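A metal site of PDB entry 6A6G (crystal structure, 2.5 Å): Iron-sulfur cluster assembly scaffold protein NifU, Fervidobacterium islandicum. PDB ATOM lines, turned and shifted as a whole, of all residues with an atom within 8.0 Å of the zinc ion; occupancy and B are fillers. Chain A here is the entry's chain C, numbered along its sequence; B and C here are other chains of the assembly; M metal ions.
The guanidinium group of Arg 120 sits close to the side-chain sulfur of Cys 62.
The side-chain hydroxyl of Ser 36 lies close to the side-chain carboxylate of Asp 39.
The backbone NH (N) of Ser 65 lies close to the side-chain sulfur (SG) of Cys 62 (3.6 Å).
A ring nitrogen (NE2) of His 354 of chain B lies close to the side-chain carboxylate (OD1) of Asp 39 (3.3 Å).
The side-chain sulfur (SG) of Cys 123 sits close to the guanidinium group (NE) of Arg 120 (3.5 Å).
O of CSS 37 lies within hydrogen-bond range of NE2 of His 356 of chain B, 3.0 Å away.
ND1 of His 354 of chain B lies within hydrogen-bond range of N of His 356 of chain B (3.2 Å).
The zinc ion is bound by OD2 of Asp 39, ND1 of His 356 of chain B, SG of Cys 62 and SG of Cys 123.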
ATOM      1  N   TYR A   6      34.213  22.738 -23.140  1.00  0.00           N
ATOM      2  CA  TYR A   6      34.615  23.017 -24.518  1.00  0.00           C
ATOM      3  C   TYR A   6      35.698  21.995 -25.028  1.00  0.00           C
ATOM      4  O   TYR A   6      36.886  22.309 -25.142  1.00  0.00           O
ATOM      5  CB  TYR A   6      35.092  24.480 -24.668  1.00  0.00           C
ATOM      6  CG  TYR A   6      33.981  25.439 -24.437  1.00  0.00           C
ATOM      7  CD1 TYR A   6      32.977  25.613 -25.395  1.00  0.00           C
ATOM      8  CD2 TYR A   6      33.860  26.093 -23.238  1.00  0.00           C
ATOM      9  CE1 TYR A   6      31.909  26.450 -25.184  1.00  0.00           C
ATOM     10  CE2 TYR A   6      32.788  26.930 -23.005  1.00  0.00           C
ATOM     11  CZ  TYR A   6      31.826  27.122 -23.969  1.00  0.00           C
ATOM     12  OH  TYR A   6      30.798  27.981 -23.704  1.00  0.00           O
ATOM     13  N   SER A  36      16.340  29.877 -25.499  1.00  0.00           N
ATOM     14  CA  SER A  36      17.752  29.625 -25.233  1.00  0.00           C
ATOM     15  C   SER A  36      18.563  30.920 -25.015  1.00  0.00           C
ATOM     16  O   SER A  36      19.754  30.936 -25.272  1.00  0.00           O
ATOM     17  CB  SER A  36      18.338  28.790 -26.375  1.00  0.00           C
ATOM     18  OG  SER A  36      19.643  28.329 -26.045  1.00  0.00           O
ATOM     19  N   CSS A  37      17.920  31.996 -24.560  1.00  0.00           N
ATOM     20  CA  CSS A  37      18.602  33.240 -24.153  1.00  0.00           C
ATOM     21  CB  CSS A  37      19.530  33.050 -22.909  1.00  0.00           C
ATOM     22  SG  CSS A  37      18.856  32.312 -21.424  1.00  0.00           S
ATOM     23  SD  CSS A  37      20.445  31.261 -20.657  1.00  0.00           S
ATOM     24  C   CSS A  37      19.378  33.937 -25.272  1.00  0.00           C
ATOM     25  O   CSS A  37      20.450  34.503 -25.037  1.00  0.00           O
ATOM     26  N   GLY A  38      18.848  33.943 -26.486  1.00  0.00           N
ATOM     27  CA  GLY A  38      19.500  34.668 -27.593  1.00  0.00           C
ATOM     28  C   GLY A  38      20.451  33.870 -28.459  1.00  0.00           C
ATOM     29  O   GLY A  38      21.349  34.422 -29.114  1.00  0.00           O
ATOM     30  N   ASP A  39      20.270  32.553 -28.460  1.00  0.00           N
ATOM     31  CA  ASP A  39      20.850  31.694 -29.467  1.00  0.00           C
ATOM     32  C   ASP A  39      19.772  31.593 -30.537  1.00  0.00           C
ATOM     33  O   ASP A  39      18.636  31.334 -30.212  1.00  0.00           O
ATOM     34  CB  ASP A  39      21.092  30.249 -28.923  1.00  0.00           C
ATOM     35  CG  ASP A  39      22.415  30.069 -28.190  1.00  0.00           C
ATOM     36  OD1 ASP A  39      23.353  30.852 -28.407  1.00  0.00           O
ATOM     37  OD2 ASP A  39      22.523  29.107 -27.399  1.00  0.00           O
ATOM     38  N   GLU A  40      20.119  31.697 -31.799  1.00  0.00           N
ATOM     39  CA  GLU A  40      19.108  31.644 -32.842  1.00  0.00           C
ATOM     40  C   GLU A  40      19.483  30.627 -33.904  1.00  0.00           C
ATOM     41  O   GLU A  40      20.629  30.570 -34.357  1.00  0.00           O
ATOM     42  CB  GLU A  40      18.970  33.022 -33.504  1.00  0.00           C
ATOM     43  CG  GLU A  40      18.728  34.177 -32.538  1.00  0.00           C
ATOM     44  CD  GLU A  40      19.184  35.546 -33.062  1.00  0.00           C
ATOM     45  OE1 GLU A  40      20.040  35.600 -34.008  1.00  0.00           O
ATOM     46  OE2 GLU A  40      18.675  36.566 -32.518  1.00  0.00           O
ATOM     47  N   HIS A  60      22.820  33.861 -34.975  1.00  0.00           N
ATOM     48  CA  HIS A  60      23.880  34.017 -34.017  1.00  0.00           C
ATOM     49  C   HIS A  60      23.693  32.983 -32.910  1.00  0.00           C
ATOM     50  O   HIS A  60      22.569  32.762 -32.437  1.00  0.00           O
ATOM     51  CB  HIS A  60      23.934  35.460 -33.506  1.00  0.00           C
ATOM     52  CG  HIS A  60      24.216  36.453 -34.582  1.00  0.00           C
ATOM     53  ND1 HIS A  60      23.229  37.164 -35.222  1.00  0.00           N
ATOM     54  CD2 HIS A  60      25.376  36.808 -35.183  1.00  0.00           C
ATOM     55  CE1 HIS A  60      23.764  37.942 -36.141  1.00  0.00           C
ATOM     56  NE2 HIS A  60      25.076  37.739 -36.144  1.00  0.00           N
ATOM     57  N   GLY A  61      24.793  32.335 -32.534  1.00  0.00           N
ATOM     58  CA  GLY A  61      24.763  31.269 -31.561  1.00  0.00           C
ATOM     59  C   GLY A  61      26.108  31.028 -30.948  1.00  0.00           C
ATOM     60  O   GLY A  61      27.148  31.130 -31.579  1.00  0.00           O
ATOM     61  N   CYS A  62      26.070  30.866 -29.654  1.00  0.00           N
ATOM     62  CA  CYS A  62      26.800  29.883 -28.920  1.00  0.00           C
ATOM     63  C   CYS A  62      27.722  28.896 -29.593  1.00  0.00           C
ATOM     64  O   CYS A  62      27.292  28.241 -30.525  1.00  0.00           O
ATOM     65  CB  CYS A  62      25.692  28.953 -28.573  1.00  0.00           C
ATOM     66  SG  CYS A  62      25.707  28.470 -26.944  1.00  0.00           S
ATOM     67  N   ALA A  63      28.880  28.635 -29.016  1.00  0.00           N
ATOM     68  CA  ALA A  63      29.742  27.557 -29.497  1.00  0.00           C
ATOM     69  C   ALA A  63      29.028  26.182 -29.428  1.00  0.00           C
ATOM     70  O   ALA A  63      29.091  25.400 -30.339  1.00  0.00           O
ATOM     71  CB  ALA A  63      31.025  27.524 -28.707  1.00  0.00           C
ATOM     72  N   ILE A  64      28.325  25.955 -28.336  1.00  0.00           N
ATOM     73  CA  ILE A  64      27.614  24.708 -28.121  1.00  0.00           C
ATOM     74  C   ILE A  64      26.403  24.540 -29.035  1.00  0.00           C
ATOM     75  O   ILE A  64      26.216  23.471 -29.618  1.00  0.00           O
ATOM     76  CB  ILE A  64      27.215  24.593 -26.645  1.00  0.00           C
ATOM     77  CG1 ILE A  64      28.497  24.395 -25.862  1.00  0.00           C
ATOM     78  CG2 ILE A  64      26.216  23.435 -26.407  1.00  0.00           C
ATOM     79  CD1 ILE A  64      28.280  24.270 -24.379  1.00  0.00           C
ATOM     80  N   SER A  65      25.585  25.588 -29.156  1.00  0.00           N
ATOM     81  CA  SER A  65      24.450  25.514 -30.087  1.00  0.00           C
ATOM     82  C   SER A  65      24.901  25.480 -31.526  1.00  0.00           C
ATOM     83  O   SER A  65      24.323  24.802 -32.327  1.00  0.00           O
ATOM     84  CB  SER A  65      23.374  26.592 -29.821  1.00  0.00           C
ATOM     85  OG  SER A  65      23.651  27.751 -30.536  1.00  0.00           O
ATOM     86  N   GLN A  66      25.963  26.164 -31.861  1.00  0.00           N
ATOM     87  CA  GLN A  66      26.470  26.097 -33.226  1.00  0.00           C
ATOM     88  C   GLN A  66      27.015  24.672 -33.562  1.00  0.00           C
ATOM     89  O   GLN A  66      26.612  24.026 -34.529  1.00  0.00           O
ATOM     90  CB  GLN A  66      27.541  27.161 -33.420  1.00  0.00           C
ATOM     91  CG  GLN A  66      27.559  27.815 -34.782  1.00  0.00           C
ATOM     92  CD  GLN A  66      27.170  29.268 -34.721  1.00  0.00           C
ATOM     93  OE1 GLN A  66      27.984  30.130 -35.025  1.00  0.00           O
ATOM     94  NE2 GLN A  66      25.930  29.555 -34.293  1.00  0.00           N
ATOM     95  N   MET A 119      22.239  24.504 -17.450  1.00  0.00           N
ATOM     96  CA  MET A 119      22.014  25.758 -18.148  1.00  0.00           C
ATOM     97  C   MET A 119      22.600  25.794 -19.546  1.00  0.00           C
ATOM     98  O   MET A 119      22.482  26.836 -20.230  1.00  0.00           O
ATOM     99  CB  MET A 119      22.554  26.919 -17.332  1.00  0.00           C
ATOM    100  CG  MET A 119      22.119  26.930 -15.867  1.00  0.00           C
ATOM    101  SD  MET A 119      20.368  27.311 -15.687  1.00  0.00           S
ATOM    102  CE  MET A 119      19.635  25.707 -15.857  1.00  0.00           C
ATOM    103  N   ARG A 120      23.226  24.700 -20.014  1.00  0.00           N
ATOM    104  CA  ARG A 120      23.707  24.665 -21.401  1.00  0.00           C
ATOM    105  C   ARG A 120      23.016  23.654 -22.273  1.00  0.00           C
ATOM    106  O   ARG A 120      23.199  23.684 -23.481  1.00  0.00           O
ATOM    107  CB  ARG A 120      25.229  24.479 -21.491  1.00  0.00           C
ATOM    108  CG  ARG A 120      26.044  25.521 -20.728  1.00  0.00           C
ATOM    109  CD  ARG A 120      25.831  26.968 -21.161  1.00  0.00           C
ATOM    110  NE  ARG A 120      26.117  27.186 -22.571  1.00  0.00           N
ATOM    111  CZ  ARG A 120      27.315  27.393 -23.116  1.00  0.00           C
ATOM    112  NH1 ARG A 120      27.427  27.599 -24.419  1.00  0.00           N
ATOM    113  NH2 ARG A 120      28.417  27.408 -22.384  1.00  0.00           N
ATOM    114  N   VAL A 121      22.202  22.812 -21.650  1.00  0.00           N
ATOM    115  CA  VAL A 121      21.316  21.868 -22.353  1.00  0.00           C
ATOM    116  C   VAL A 121      20.452  22.579 -23.416  1.00  0.00           C
ATOM    117  O   VAL A 121      20.316  22.101 -24.540  1.00  0.00           O
ATOM    118  CB  VAL A 121      20.423  21.147 -21.316  1.00  0.00           C
ATOM    119  CG1 VAL A 121      19.202  20.466 -21.950  1.00  0.00           C
ATOM    120  CG2 VAL A 121      21.254  20.131 -20.522  1.00  0.00           C
ATOM    121  N   LYS A 122      19.845  23.709 -23.040  1.00  0.00           N
ATOM    122  CA  LYS A 122      19.035  24.498 -23.960  1.00  0.00           C
ATOM    123  C   LYS A 122      19.851  24.824 -25.207  1.00  0.00           C
ATOM    124  O   LYS A 122      19.377  24.672 -26.297  1.00  0.00           O
ATOM    125  CB  LYS A 122      18.485  25.798 -23.289  1.00  0.00           C
ATOM    126  CG  LYS A 122      19.582  26.805 -22.831  1.00  0.00           C
ATOM    127  CD  LYS A 122      19.069  27.941 -21.941  1.00  0.00           C
ATOM    128  CE  LYS A 122      18.425  27.438 -20.649  1.00  0.00           C
ATOM    129  NZ  LYS A 122      18.817  28.297 -19.504  1.00  0.00           N
ATOM    130  N   CYS A 123      21.105  25.241 -25.024  1.00  0.00           N
ATOM    131  CA  CYS A 123      21.971  25.561 -26.161  1.00  0.00           C
ATOM    132  C   CYS A 123      22.158  24.335 -27.061  1.00  0.00           C
ATOM    133  O   CYS A 123      22.079  24.448 -28.278  1.00  0.00           O
ATOM    134  CB  CYS A 123      23.320  26.113 -25.672  1.00  0.00           C
ATOM    135  SG  CYS A 123      23.223  27.451 -24.445  1.00  0.00           S
ATOM    136  N   PHE A 124      22.362  23.163 -26.462  1.00  0.00           N
ATOM    137  CA  PHE A 124      22.487  21.954 -27.296  1.00  0.00           C
ATOM    138  C   PHE A 124      21.187  21.597 -28.029  1.00  0.00           C
ATOM    139  O   PHE A 124      21.198  21.199 -29.219  1.00  0.00           O
ATOM    140  CB  PHE A 124      22.919  20.759 -26.458  1.00  0.00           C
ATOM    141  CG  PHE A 124      22.811  19.440 -27.201  1.00  0.00           C
ATOM    142  CD1 PHE A 124      23.801  19.036 -28.084  1.00  0.00           C
ATOM    143  CD2 PHE A 124      21.714  18.637 -27.015  1.00  0.00           C
ATOM    144  CE1 PHE A 124      23.711  17.841 -28.758  1.00  0.00           C
ATOM    145  CE2 PHE A 124      21.603  17.438 -27.684  1.00  0.00           C
ATOM    146  CZ  PHE A 124      22.612  17.042 -28.559  1.00  0.00           C
ATOM    147  N   LEU A 126      18.391  23.400 -28.772  1.00  0.00           N
ATOM    148  CA  LEU A 126      17.806  24.392 -29.678  1.00  0.00           C
ATOM    149  C   LEU A 126      17.629  23.900 -31.115  1.00  0.00           C
ATOM    150  O   LEU A 126      16.522  23.932 -31.607  1.00  0.00           O
ATOM    151  CB  LEU A 126      18.546  25.729 -29.669  1.00  0.00           C
ATOM    152  CG  LEU A 126      18.032  26.718 -30.735  1.00  0.00           C
ATOM    153  CD1 LEU A 126      16.582  27.071 -30.429  1.00  0.00           C
ATOM    154  CD2 LEU A 126      18.886  27.971 -30.850  1.00  0.00           C
ATOM    155  N   HIS B 354      30.389  34.613 -28.439  1.00  0.00           N
ATOM    156  CA  HIS B 354      28.989  34.718 -27.989  1.00  0.00           C
ATOM    157  C   HIS B 354      28.880  34.850 -26.465  1.00  0.00           C
ATOM    158  O   HIS B 354      29.640  34.225 -25.699  1.00  0.00           O
ATOM    159  CB  HIS B 354      28.198  33.498 -28.463  1.00  0.00           C
ATOM    160  CG  HIS B 354      26.714  33.649 -28.361  1.00  0.00           C
ATOM    161  ND1 HIS B 354      26.027  33.398 -27.198  1.00  0.00           N
ATOM    162  CD2 HIS B 354      25.776  33.947 -29.287  1.00  0.00           C
ATOM    163  CE1 HIS B 354      24.725  33.572 -27.403  1.00  0.00           C
ATOM    164  NE2 HIS B 354      24.546  33.892 -28.669  1.00  0.00           N
ATOM    165  N   PRO B 355      27.936  35.684 -26.002  1.00  0.00           N
ATOM    166  CA  PRO B 355      27.746  35.916 -24.579  1.00  0.00           C
ATOM    167  C   PRO B 355      27.645  34.669 -23.726  1.00  0.00           C
ATOM    168  O   PRO B 355      28.173  34.646 -22.613  1.00  0.00           O
ATOM    169  CB  PRO B 355      26.432  36.678 -24.526  1.00  0.00           C
ATOM    170  CG  PRO B 355      26.430  37.443 -25.777  1.00  0.00           C
ATOM    171  CD  PRO B 355      27.086  36.570 -26.810  1.00  0.00           C
ATOM    172  N   HIS B 356      26.976  33.622 -24.188  1.00  0.00           N
ATOM    173  CA  HIS B 356      26.933  32.383 -23.365  1.00  0.00           C
ATOM    174  C   HIS B 356      28.290  31.792 -23.103  1.00  0.00           C
ATOM    175  O   HIS B 356      28.587  31.387 -21.983  1.00  0.00           O
ATOM    176  CB  HIS B 356      26.089  31.308 -23.979  1.00  0.00           C
ATOM    177  CG  HIS B 356      24.691  31.744 -24.250  1.00  0.00           C
ATOM    178  ND1 HIS B 356      23.792  30.952 -24.923  1.00  0.00           N
ATOM    179  CD2 HIS B 356      24.053  32.911 -23.976  1.00  0.00           C
ATOM    180  CE1 HIS B 356      22.651  31.597 -25.034  1.00  0.00           C
ATOM    181  NE2 HIS B 356      22.779  32.788 -24.456  1.00  0.00           N
ATOM    182  N   ASP B 357      29.137  31.789 -24.115  1.00  0.00           N
ATOM    183  CA  ASP B 357      30.442  31.208 -23.949  1.00  0.00           C
ATOM    184  C   ASP B 357      31.284  32.060 -23.027  1.00  0.00           C
ATOM    185  O   ASP B 357      31.999  31.546 -22.179  1.00  0.00           O
ATOM    186  CB  ASP B 357      31.092  31.001 -25.324  1.00  0.00           C
ATOM    187  CG  ASP B 357      30.227  30.109 -26.237  1.00  0.00           C
ATOM    188  OD1 ASP B 357      29.739  29.068 -25.790  1.00  0.00           O
ATOM    189  OD2 ASP B 357      30.011  30.469 -27.410  1.00  0.00           O
ATOM    190  N   SER B 372      24.124  36.746 -19.433  1.00  0.00           N
ATOM    191  CA  SER B 372      24.384  36.656 -20.836  1.00  0.00           C
ATOM    192  C   SER B 372      23.042  36.420 -21.549  1.00  0.00           C
ATOM    193  O   SER B 372      22.377  35.454 -21.235  1.00  0.00           O
ATOM    194  CB  SER B 372      25.343  35.503 -21.085  1.00  0.00           C
ATOM    195  OG  SER B 372      24.733  34.245 -20.809  1.00  0.00           O
ATOM    196  N   VAL C  68      23.955  31.334 -16.835  1.00  0.00           N
ATOM    197  CA  VAL C  68      24.709  30.078 -16.869  1.00  0.00           C
ATOM    198  C   VAL C  68      25.704  29.848 -15.713  1.00  0.00           C
ATOM    199  O   VAL C  68      26.372  28.798 -15.657  1.00  0.00           O
ATOM    200  CB  VAL C  68      25.424  29.906 -18.212  1.00  0.00           C
ATOM    201  CG1 VAL C  68      24.413  30.046 -19.350  1.00  0.00           C
ATOM    202  CG2 VAL C  68      26.606  30.873 -18.353  1.00  0.00           C
HETATM  203 ZN    ZN M   1      23.791  29.143 -25.946  1.00  0.00          ZN
